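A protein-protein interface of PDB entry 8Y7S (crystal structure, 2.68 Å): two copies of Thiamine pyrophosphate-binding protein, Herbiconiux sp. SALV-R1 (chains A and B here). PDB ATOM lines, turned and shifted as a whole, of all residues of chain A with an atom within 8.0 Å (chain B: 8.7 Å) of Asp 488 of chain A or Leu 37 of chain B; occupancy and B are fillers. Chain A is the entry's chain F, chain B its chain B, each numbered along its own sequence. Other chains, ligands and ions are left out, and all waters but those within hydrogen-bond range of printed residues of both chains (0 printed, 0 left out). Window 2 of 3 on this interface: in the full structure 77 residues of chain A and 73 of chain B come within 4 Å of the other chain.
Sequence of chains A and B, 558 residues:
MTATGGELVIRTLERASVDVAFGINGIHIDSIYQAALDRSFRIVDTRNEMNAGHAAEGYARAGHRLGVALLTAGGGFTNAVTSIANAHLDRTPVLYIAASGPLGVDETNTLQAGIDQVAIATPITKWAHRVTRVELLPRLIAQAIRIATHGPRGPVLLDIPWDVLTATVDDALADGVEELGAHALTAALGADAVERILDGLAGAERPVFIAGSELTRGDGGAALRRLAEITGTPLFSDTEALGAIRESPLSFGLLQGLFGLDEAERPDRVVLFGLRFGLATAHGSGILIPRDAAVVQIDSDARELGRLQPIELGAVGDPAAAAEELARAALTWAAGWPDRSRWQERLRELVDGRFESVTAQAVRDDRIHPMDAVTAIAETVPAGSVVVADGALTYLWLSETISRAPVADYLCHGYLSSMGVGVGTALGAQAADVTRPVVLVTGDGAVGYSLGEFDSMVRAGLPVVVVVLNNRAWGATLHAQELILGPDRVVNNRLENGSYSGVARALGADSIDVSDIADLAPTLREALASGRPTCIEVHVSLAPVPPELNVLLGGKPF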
ATOM      1  N   GLN A 481      -5.907 -25.273   3.489  1.00  0.00           N
ATOM      2  CA  GLN A 481      -6.969 -25.090   4.469  1.00  0.00           C
ATOM      3  C   GLN A 481      -7.808 -23.864   4.133  1.00  0.00           C
ATOM      4  O   GLN A 481      -9.042 -23.936   4.093  1.00  0.00           O
ATOM      5  CB  GLN A 481      -6.382 -24.983   5.871  1.00  0.00           C
ATOM      6  CG  GLN A 481      -5.663 -26.232   6.321  1.00  0.00           C
ATOM      7  CD  GLN A 481      -4.969 -26.044   7.646  1.00  0.00           C
ATOM      8  OE1 GLN A 481      -4.400 -24.987   7.913  1.00  0.00           O
ATOM      9  NE2 GLN A 481      -5.010 -27.068   8.488  1.00  0.00           N
ATOM     10  N   GLU A 482      -7.154 -22.726   3.878  1.00  0.00           N
ATOM     11  CA  GLU A 482      -7.900 -21.495   3.636  1.00  0.00           C
ATOM     12  C   GLU A 482      -8.716 -21.567   2.348  1.00  0.00           C
ATOM     13  O   GLU A 482      -9.908 -21.233   2.341  1.00  0.00           O
ATOM     14  CB  GLU A 482      -6.955 -20.296   3.597  1.00  0.00           C
ATOM     15  CG  GLU A 482      -7.663 -19.019   3.165  1.00  0.00           C
ATOM     16  CD  GLU A 482      -7.253 -17.804   3.971  1.00  0.00           C
ATOM     17  OE1 GLU A 482      -6.487 -17.954   4.950  1.00  0.00           O
ATOM     18  OE2 GLU A 482      -7.713 -16.697   3.631  1.00  0.00           O
ATOM     19  N   LEU A 485     -11.212 -24.936   2.749  1.00  0.00           N
ATOM     20  CA  LEU A 485     -12.110 -24.940   3.899  1.00  0.00           C
ATOM     21  C   LEU A 485     -12.469 -23.559   4.441  1.00  0.00           C
ATOM     22  O   LEU A 485     -13.450 -23.449   5.180  1.00  0.00           O
ATOM     23  CB  LEU A 485     -11.499 -25.762   5.040  1.00  0.00           C
ATOM     24  CG  LEU A 485     -10.983 -27.155   4.672  1.00  0.00           C
ATOM     25  CD1 LEU A 485     -10.388 -27.839   5.896  1.00  0.00           C
ATOM     26  CD2 LEU A 485     -12.102 -28.004   4.057  1.00  0.00           C
ATOM     27  N   GLY A 486     -11.729 -22.507   4.100  1.00  0.00           N
ATOM     28  CA  GLY A 486     -12.036 -21.192   4.616  1.00  0.00           C
ATOM     29  C   GLY A 486     -11.033 -20.682   5.633  1.00  0.00           C
ATOM     30  O   GLY A 486     -10.286 -21.450   6.247  1.00  0.00           O
ATOM     31  N   PRO A 487     -11.020 -19.360   5.849  1.00  0.00           N
ATOM     32  CA  PRO A 487      -9.969 -18.770   6.692  1.00  0.00           C
ATOM     33  C   PRO A 487     -10.100 -19.128   8.160  1.00  0.00           C
ATOM     34  O   PRO A 487      -9.100 -19.087   8.884  1.00  0.00           O
ATOM     35  CB  PRO A 487     -10.141 -17.261   6.463  1.00  0.00           C
ATOM     36  CG  PRO A 487     -11.094 -17.143   5.274  1.00  0.00           C
ATOM     37  CD  PRO A 487     -11.971 -18.339   5.386  1.00  0.00           C
ATOM     38  N   ASP A 488     -11.308 -19.449   8.627  1.00  0.00           N
ATOM     39  CA  ASP A 488     -11.488 -19.890  10.004  1.00  0.00           C
ATOM     40  C   ASP A 488     -10.910 -21.277  10.258  1.00  0.00           C
ATOM     41  O   ASP A 488     -10.706 -21.641  11.420  1.00  0.00           O
ATOM     42  CB  ASP A 488     -12.974 -19.868  10.383  1.00  0.00           C
ATOM     43  CG  ASP A 488     -13.860 -20.538   9.342  1.00  0.00           C
ATOM     44  OD1 ASP A 488     -13.717 -20.236   8.136  1.00  0.00           O
ATOM     45  OD2 ASP A 488     -14.712 -21.366   9.735  1.00  0.00           O
ATOM     46  N   ARG A 489     -10.676 -22.070   9.212  1.00  0.00           N
ATOM     47  CA  ARG A 489     -10.197 -23.440   9.376  1.00  0.00           C
ATOM     48  C   ARG A 489      -8.680 -23.574   9.316  1.00  0.00           C
ATOM     49  O   ARG A 489      -8.173 -24.698   9.399  1.00  0.00           O
ATOM     50  CB  ARG A 489     -10.835 -24.360   8.334  1.00  0.00           C
ATOM     51  CG  ARG A 489     -12.324 -24.140   8.124  1.00  0.00           C
ATOM     52  CD  ARG A 489     -13.096 -24.453   9.390  1.00  0.00           C
ATOM     53  NE  ARG A 489     -12.580 -25.661  10.015  1.00  0.00           N
ATOM     54  CZ  ARG A 489     -13.078 -26.221  11.107  1.00  0.00           C
ATOM     55  NH1 ARG A 489     -13.961 -25.596  11.862  1.00  0.00           N
ATOM     56  NH2 ARG A 489     -12.642 -27.423  11.473  1.00  0.00           N
ATOM     57  N   VAL A 490      -7.943 -22.474   9.167  1.00  0.00           N
ATOM     58  CA  VAL A 490      -6.488 -22.550   9.162  1.00  0.00           C
ATOM     59  C   VAL A 490      -6.014 -22.916  10.561  1.00  0.00           C
ATOM     60  O   VAL A 490      -6.356 -22.243  11.538  1.00  0.00           O
ATOM     61  CB  VAL A 490      -5.894 -21.210   8.699  1.00  0.00           C
ATOM     62  CG1 VAL A 490      -4.413 -21.111   9.046  1.00  0.00           C
ATOM     63  CG2 VAL A 490      -6.125 -21.011   7.205  1.00  0.00           C
ATOM     64  N   VAL A 491      -5.222 -23.980  10.670  1.00  0.00           N
ATOM     65  CA  VAL A 491      -4.753 -24.422  11.980  1.00  0.00           C
ATOM     66  C   VAL A 491      -3.425 -25.152  11.823  1.00  0.00           C
ATOM     67  O   VAL A 491      -3.193 -25.854  10.835  1.00  0.00           O
ATOM     68  CB  VAL A 491      -5.813 -25.302  12.687  1.00  0.00           C
ATOM     69  CG1 VAL A 491      -6.003 -26.615  11.948  1.00  0.00           C
ATOM     70  CG2 VAL A 491      -5.431 -25.537  14.150  1.00  0.00           C
ATOM     71  N   ASN A 492      -2.540 -24.945  12.799  1.00  0.00           N
ATOM     72  CA  ASN A 492      -1.246 -25.621  12.878  1.00  0.00           C
ATOM     73  C   ASN A 492      -0.356 -25.337  11.670  1.00  0.00           C
ATOM     74  O   ASN A 492       0.439 -26.187  11.270  1.00  0.00           O
ATOM     75  CB  ASN A 492      -1.419 -27.130  13.060  1.00  0.00           C
ATOM     76  CG  ASN A 492      -1.785 -27.502  14.479  1.00  0.00           C
ATOM     77  OD1 ASN A 492      -2.939 -27.801  14.772  1.00  0.00           O
ATOM     78  ND2 ASN A 492      -0.802 -27.478  15.367  1.00  0.00           N
ATOM     79  N   ILE B  10      -9.834 -38.954  16.394  1.00  0.00           N
ATOM     80  CA  ILE B  10      -9.808 -38.084  17.608  1.00  0.00           C
ATOM     81  C   ILE B  10     -10.705 -38.691  18.699  1.00  0.00           C
ATOM     82  O   ILE B  10     -10.285 -38.699  19.868  1.00  0.00           O
ATOM     83  CB  ILE B  10     -10.211 -36.641  17.246  1.00  0.00           C
ATOM     84  CG1 ILE B  10      -9.247 -36.038  16.233  1.00  0.00           C
ATOM     85  CG2 ILE B  10     -10.330 -35.766  18.492  1.00  0.00           C
ATOM     86  CD1 ILE B  10      -7.856 -35.794  16.785  1.00  0.00           C
ATOM     87  N   GLU B  14      -9.555 -39.621  22.254  1.00  0.00           N
ATOM     88  CA  GLU B  14     -10.194 -39.088  23.454  1.00  0.00           C
ATOM     89  C   GLU B  14     -10.534 -40.208  24.432  1.00  0.00           C
ATOM     90  O   GLU B  14     -10.241 -40.111  25.630  1.00  0.00           O
ATOM     91  CB  GLU B  14     -11.447 -38.297  23.086  1.00  0.00           C
ATOM     92  CG  GLU B  14     -11.183 -36.962  22.391  1.00  0.00           C
ATOM     93  CD  GLU B  14     -12.440 -36.377  21.746  1.00  0.00           C
ATOM     94  OE1 GLU B  14     -13.439 -37.117  21.586  1.00  0.00           O
ATOM     95  OE2 GLU B  14     -12.427 -35.176  21.401  1.00  0.00           O
ATOM     96  N   ASP B  30      -4.961 -33.765   7.063  1.00  0.00           N
ATOM     97  CA  ASP B  30      -5.630 -32.587   7.620  1.00  0.00           C
ATOM     98  C   ASP B  30      -6.986 -32.918   8.246  1.00  0.00           C
ATOM     99  O   ASP B  30      -7.449 -32.197   9.141  1.00  0.00           O
ATOM    100  CB  ASP B  30      -5.796 -31.512   6.549  1.00  0.00           C
ATOM    101  CG  ASP B  30      -6.041 -30.131   7.147  1.00  0.00           C
ATOM    102  OD1 ASP B  30      -5.303 -29.747   8.079  1.00  0.00           O
ATOM    103  OD2 ASP B  30      -6.977 -29.436   6.696  1.00  0.00           O
ATOM    104  N   SER B  31      -7.652 -33.973   7.772  1.00  0.00           N
ATOM    105  CA  SER B  31      -8.942 -34.351   8.342  1.00  0.00           C
ATOM    106  C   SER B  31      -8.838 -34.609   9.841  1.00  0.00           C
ATOM    107  O   SER B  31      -9.794 -34.359  10.583  1.00  0.00           O
ATOM    108  CB  SER B  31      -9.489 -35.581   7.621  1.00  0.00           C
ATOM    109  OG  SER B  31     -10.697 -36.015   8.214  1.00  0.00           O
ATOM    110  N   ILE B  32      -7.697 -35.129  10.301  1.00  0.00           N
ATOM    111  CA  ILE B  32      -7.474 -35.293  11.734  1.00  0.00           C
ATOM    112  C   ILE B  32      -7.361 -33.933  12.414  1.00  0.00           C
ATOM    113  O   ILE B  32      -7.898 -33.726  13.508  1.00  0.00           O
ATOM    114  CB  ILE B  32      -6.218 -36.151  11.985  1.00  0.00           C
ATOM    115  CG1 ILE B  32      -6.400 -37.551  11.395  1.00  0.00           C
ATOM    116  CG2 ILE B  32      -5.894 -36.212  13.470  1.00  0.00           C
ATOM    117  CD1 ILE B  32      -5.377 -38.577  11.874  1.00  0.00           C
ATOM    118  N   TYR B  33      -6.645 -32.996  11.784  1.00  0.00           N
ATOM    119  CA  TYR B  33      -6.471 -31.661  12.352  1.00  0.00           C
ATOM    120  C   TYR B  33      -7.791 -30.904  12.396  1.00  0.00           C
ATOM    121  O   TYR B  33      -8.093 -30.216  13.380  1.00  0.00           O
ATOM    122  CB  TYR B  33      -5.435 -30.884  11.545  1.00  0.00           C
ATOM    123  CG  TYR B  33      -4.024 -31.329  11.803  1.00  0.00           C
ATOM    124  CD1 TYR B  33      -3.554 -32.540  11.318  1.00  0.00           C
ATOM    125  CD2 TYR B  33      -3.162 -30.548  12.541  1.00  0.00           C
ATOM    126  CE1 TYR B  33      -2.254 -32.952  11.561  1.00  0.00           C
ATOM    127  CE2 TYR B  33      -1.866 -30.948  12.788  1.00  0.00           C
ATOM    128  CZ  TYR B  33      -1.413 -32.144  12.297  1.00  0.00           C
ATOM    129  OH  TYR B  33      -0.117 -32.525  12.556  1.00  0.00           O
ATOM    130  N   GLN B  34      -8.583 -31.009  11.330  1.00  0.00           N
ATOM    131  CA  GLN B  34      -9.891 -30.369  11.321  1.00  0.00           C
ATOM    132  C   GLN B  34     -10.774 -30.909  12.440  1.00  0.00           C
ATOM    133  O   GLN B  34     -11.475 -30.144  13.117  1.00  0.00           O
ATOM    134  CB  GLN B  34     -10.539 -30.559   9.952  1.00  0.00           C
ATOM    135  CG  GLN B  34      -9.865 -29.734   8.874  1.00  0.00           C
ATOM    136  CD  GLN B  34      -9.802 -28.261   9.235  1.00  0.00           C
ATOM    137  OE1 GLN B  34     -10.811 -27.664   9.610  1.00  0.00           O
ATOM    138  NE2 GLN B  34      -8.613 -27.670   9.131  1.00  0.00           N
ATOM    139  N   ALA B  35     -10.746 -32.224  12.656  1.00  0.00           N
ATOM    140  CA  ALA B  35     -11.507 -32.809  13.753  1.00  0.00           C
ATOM    141  C   ALA B  35     -10.985 -32.320  15.096  1.00  0.00           C
ATOM    142  O   ALA B  35     -11.761 -32.072  16.022  1.00  0.00           O
ATOM    143  CB  ALA B  35     -11.444 -34.331  13.680  1.00  0.00           C
ATOM    144  N   ALA B  36      -9.662 -32.203  15.221  1.00  0.00           N
ATOM    145  CA  ALA B  36      -9.062 -31.700  16.450  1.00  0.00           C
ATOM    146  C   ALA B  36      -9.454 -30.253  16.712  1.00  0.00           C
ATOM    147  O   ALA B  36      -9.564 -29.845  17.873  1.00  0.00           O
ATOM    148  CB  ALA B  36      -7.541 -31.842  16.391  1.00  0.00           C
ATOM    149  N   LEU B  37      -9.616 -29.455  15.652  1.00  0.00           N
ATOM    150  CA  LEU B  37     -10.049 -28.070  15.819  1.00  0.00           C
ATOM    151  C   LEU B  37     -11.452 -27.996  16.416  1.00  0.00           C
ATOM    152  O   LEU B  37     -11.683 -27.262  17.384  1.00  0.00           O
ATOM    153  CB  LEU B  37      -9.994 -27.327  14.481  1.00  0.00           C
ATOM    154  CG  LEU B  37     -10.376 -25.841  14.484  1.00  0.00           C
ATOM    155  CD1 LEU B  37      -9.457 -25.033  15.401  1.00  0.00           C
ATOM    156  CD2 LEU B  37     -10.364 -25.264  13.064  1.00  0.00           C
ATOM    157  N   ASP B  38     -12.404 -28.746  15.853  1.00  0.00           N
ATOM    158  CA  ASP B  38     -13.766 -28.711  16.387  1.00  0.00           C
ATOM    159  C   ASP B  38     -13.852 -29.277  17.800  1.00  0.00           C
ATOM    160  O   ASP B  38     -14.544 -28.715  18.661  1.00  0.00           O
ATOM    161  CB  ASP B  38     -14.732 -29.496  15.492  1.00  0.00           C
ATOM    162  CG  ASP B  38     -14.630 -29.134  14.010  1.00  0.00           C
ATOM    163  OD1 ASP B  38     -14.335 -27.974  13.670  1.00  0.00           O
ATOM    164  OD2 ASP B  38     -14.893 -30.027  13.171  1.00  0.00           O
ATOM    165  N   ARG B  39     -13.183 -30.409  18.059  1.00  0.00           N
ATOM    166  CA  ARG B  39     -13.280 -31.166  19.323  1.00  0.00           C
ATOM    167  C   ARG B  39     -12.281 -30.601  20.316  1.00  0.00           C
ATOM    168  O   ARG B  39     -12.267 -31.084  21.495  1.00  0.00           O
ATOM    169  CB  ARG B  39     -13.013 -32.626  19.060  1.00  0.00           C
ATOM    170  CG  ARG B  39     -14.017 -33.180  18.182  1.00  0.00           C
ATOM    171  CD  ARG B  39     -14.025 -34.651  18.342  1.00  0.00           C
ATOM    172  NE  ARG B  39     -14.572 -35.059  19.626  1.00  0.00           N
ATOM    173  CZ  ARG B  39     -15.825 -35.452  19.795  1.00  0.00           C
ATOM    174  NH1 ARG B  39     -16.588 -35.773  18.765  1.00  0.00           N
ATOM    175  NH2 ARG B  39     -16.288 -35.636  21.027  1.00  0.00           N
ATOM    176  N   SER B  40     -11.484 -29.610  19.848  1.00  0.00           N
ATOM    177  CA  SER B  40     -10.646 -28.818  20.678  1.00  0.00           C
ATOM    178  C   SER B  40      -9.577 -29.627  21.384  1.00  0.00           C
ATOM    179  O   SER B  40      -9.241 -29.368  22.562  1.00  0.00           O
ATOM    180  CB  SER B  40     -11.408 -27.842  21.574  1.00  0.00           C
ATOM    181  OG  SER B  40     -10.937 -27.584  22.924  1.00  0.00           O
ATOM    182  N   PHE B  41      -9.174 -30.697  20.657  1.00  0.00           N
ATOM    183  CA  PHE B  41      -7.981 -31.557  20.834  1.00  0.00           C
ATOM    184  C   PHE B  41      -6.699 -30.821  20.392  1.00  0.00           C
ATOM    185  O   PHE B  41      -6.613 -30.229  19.296  1.00  0.00           O
ATOM    186  CB  PHE B  41      -8.159 -32.810  19.967  1.00  0.00           C
ATOM    187  CG  PHE B  41      -7.162 -33.925  20.282  1.00  0.00           C
ATOM    188  CD1 PHE B  41      -5.896 -33.957  19.716  1.00  0.00           C
ATOM    189  CD2 PHE B  41      -7.520 -34.956  21.141  1.00  0.00           C
ATOM    190  CE1 PHE B  41      -4.991 -34.998  20.012  1.00  0.00           C
ATOM    191  CE2 PHE B  41      -6.621 -35.999  21.447  1.00  0.00           C
ATOM    192  CZ  PHE B  41      -5.354 -36.014  20.877  1.00  0.00           C
ATOM    193  N   ARG B  42      -5.667 -30.960  21.202  1.00  0.00           N
ATOM    194  CA  ARG B  42      -4.453 -30.175  21.043  1.00  0.00           C
ATOM    195  C   ARG B  42      -3.411 -30.959  20.254  1.00  0.00           C
ATOM    196  O   ARG B  42      -3.017 -32.065  20.648  1.00  0.00           O
ATOM    197  CB  ARG B  42      -3.871 -29.754  22.394  1.00  0.00           C
ATOM    198  CG  ARG B  42      -2.522 -29.096  22.219  1.00  0.00           C
ATOM    199  CD  ARG B  42      -1.983 -28.397  23.455  1.00  0.00           C
ATOM    200  NE  ARG B  42      -0.811 -27.604  23.090  1.00  0.00           N
ATOM    201  CZ  ARG B  42      -0.002 -26.985  23.942  1.00  0.00           C
ATOM    202  NH1 ARG B  42      -0.201 -27.029  25.248  1.00  0.00           N
ATOM    203  NH2 ARG B  42       1.044 -26.312  23.468  1.00  0.00           N
ATOM    204  N   ILE B  43      -2.955 -30.364  19.160  1.00  0.00           N
ATOM    205  CA  ILE B  43      -1.845 -30.871  18.375  1.00  0.00           C
ATOM    206  C   ILE B  43      -0.721 -29.844  18.437  1.00  0.00           C
ATOM    207  O   ILE B  43      -0.908 -28.686  18.048  1.00  0.00           O
ATOM    208  CB  ILE B  43      -2.256 -31.145  16.923  1.00  0.00           C
ATOM    209  CG1 ILE B  43      -3.357 -32.200  16.873  1.00  0.00           C
ATOM    210  CG2 ILE B  43      -1.062 -31.592  16.109  1.00  0.00           C
ATOM    211  CD1 ILE B  43      -4.009 -32.295  15.527  1.00  0.00           C
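The side-chain amide nitrogen (NE2) of Gln 481 of chain A is in hydrogen-bond range of the side-chain carboxylate (OD1) of Asp 30 of chain B (2.7 Å). OE1 of Gln 34 of chain B is in hydrogen-bond range of NH2 of Arg 489 of chain A, at 2.6 Å. The guanidinium group (NH2) of Arg 489 of chain A is in salt-bridge range of the side-chain carboxylate (OD1) of Asp 38 of chain B, at 2.8 Å. The backbone carbonyl oxygen (O) of Ile 43 of chain B lies within hydrogen-bond range of the side-chain amide nitrogen (ND2) of Asn 492 of chain A (2.9 Å).
OD2 of Asp 30 of chain B lies within hydrogen-bond range of NE2 of Gln 34 of chain B (3.4 Å). O of Gln 481 of chain A lies within hydrogen-bond range of N of Gly 486 of chain A (3.0 Å). The backbone NH (N) of Val 491 of chain A lies within hydrogen-bond range of the side-chain amide oxygen (OE1) of Gln 481 of chain A (3.0 Å).
Gln 481 of chain A touches Gln 34 of chain B. Leu 485 of chain A touches Asp 30 of chain B. Gln 34 of chain B touches Leu 485 of chain A (CD to CD1, 3.4 Å). Leu 37 of chain B touches Asp 488 of chain A. CD2 of Leu 37 of chain B touches CZ of Arg 489 of chain A (3.5 Å). Val 491 of chain A touches Gln 34 of chain B (CG1 to NE2, 3.98 Å). Asn 492 of chain A touches Tyr 33 of chain B (OD1 to CD2, 3.5 Å).
Of the printed residues of chain B, Asp 488 of chain A touches Leu 37. Of the printed residues of chain A, Leu 37 of chain B touches Asp 488 (3.99 Å) and Arg 489 (3.5 Å). Ala 36 of chain B touches none of the printed residues of chain A. Of the printed residues of chain B, Leu 485 of chain A touches Asp 30 and Gln 34. Of the printed residues of chain A, Gln 34 of chain B touches Gln 481, Leu 485, Arg 489 and Val 491. Of the printed residues of chain B, Val 491 of chain A touches Gln 34 (3.98 Å). Of the printed residues of chain A, Asp 38 of chain B touches Arg 489 (2.8 Å). Phe 41 of chain B touches none of the printed residues of chain A. Ile 32 of chain B touches none of the printed residues of chain A. The nearest printed residue of chain B that does not touch Asp 488 of chain A is Gln 34 of chain B (6.3 Å).
Of the 16 printed residues of chain B, 6 touch a printed residue of chain A. Hydrophobic or aromatic side chains of chain B within 4 Å of the printed part of chain A: Tyr 33 and Leu 37. Among the printed residues, 11 pairs touch across the chains.
No position is printed for both chains.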
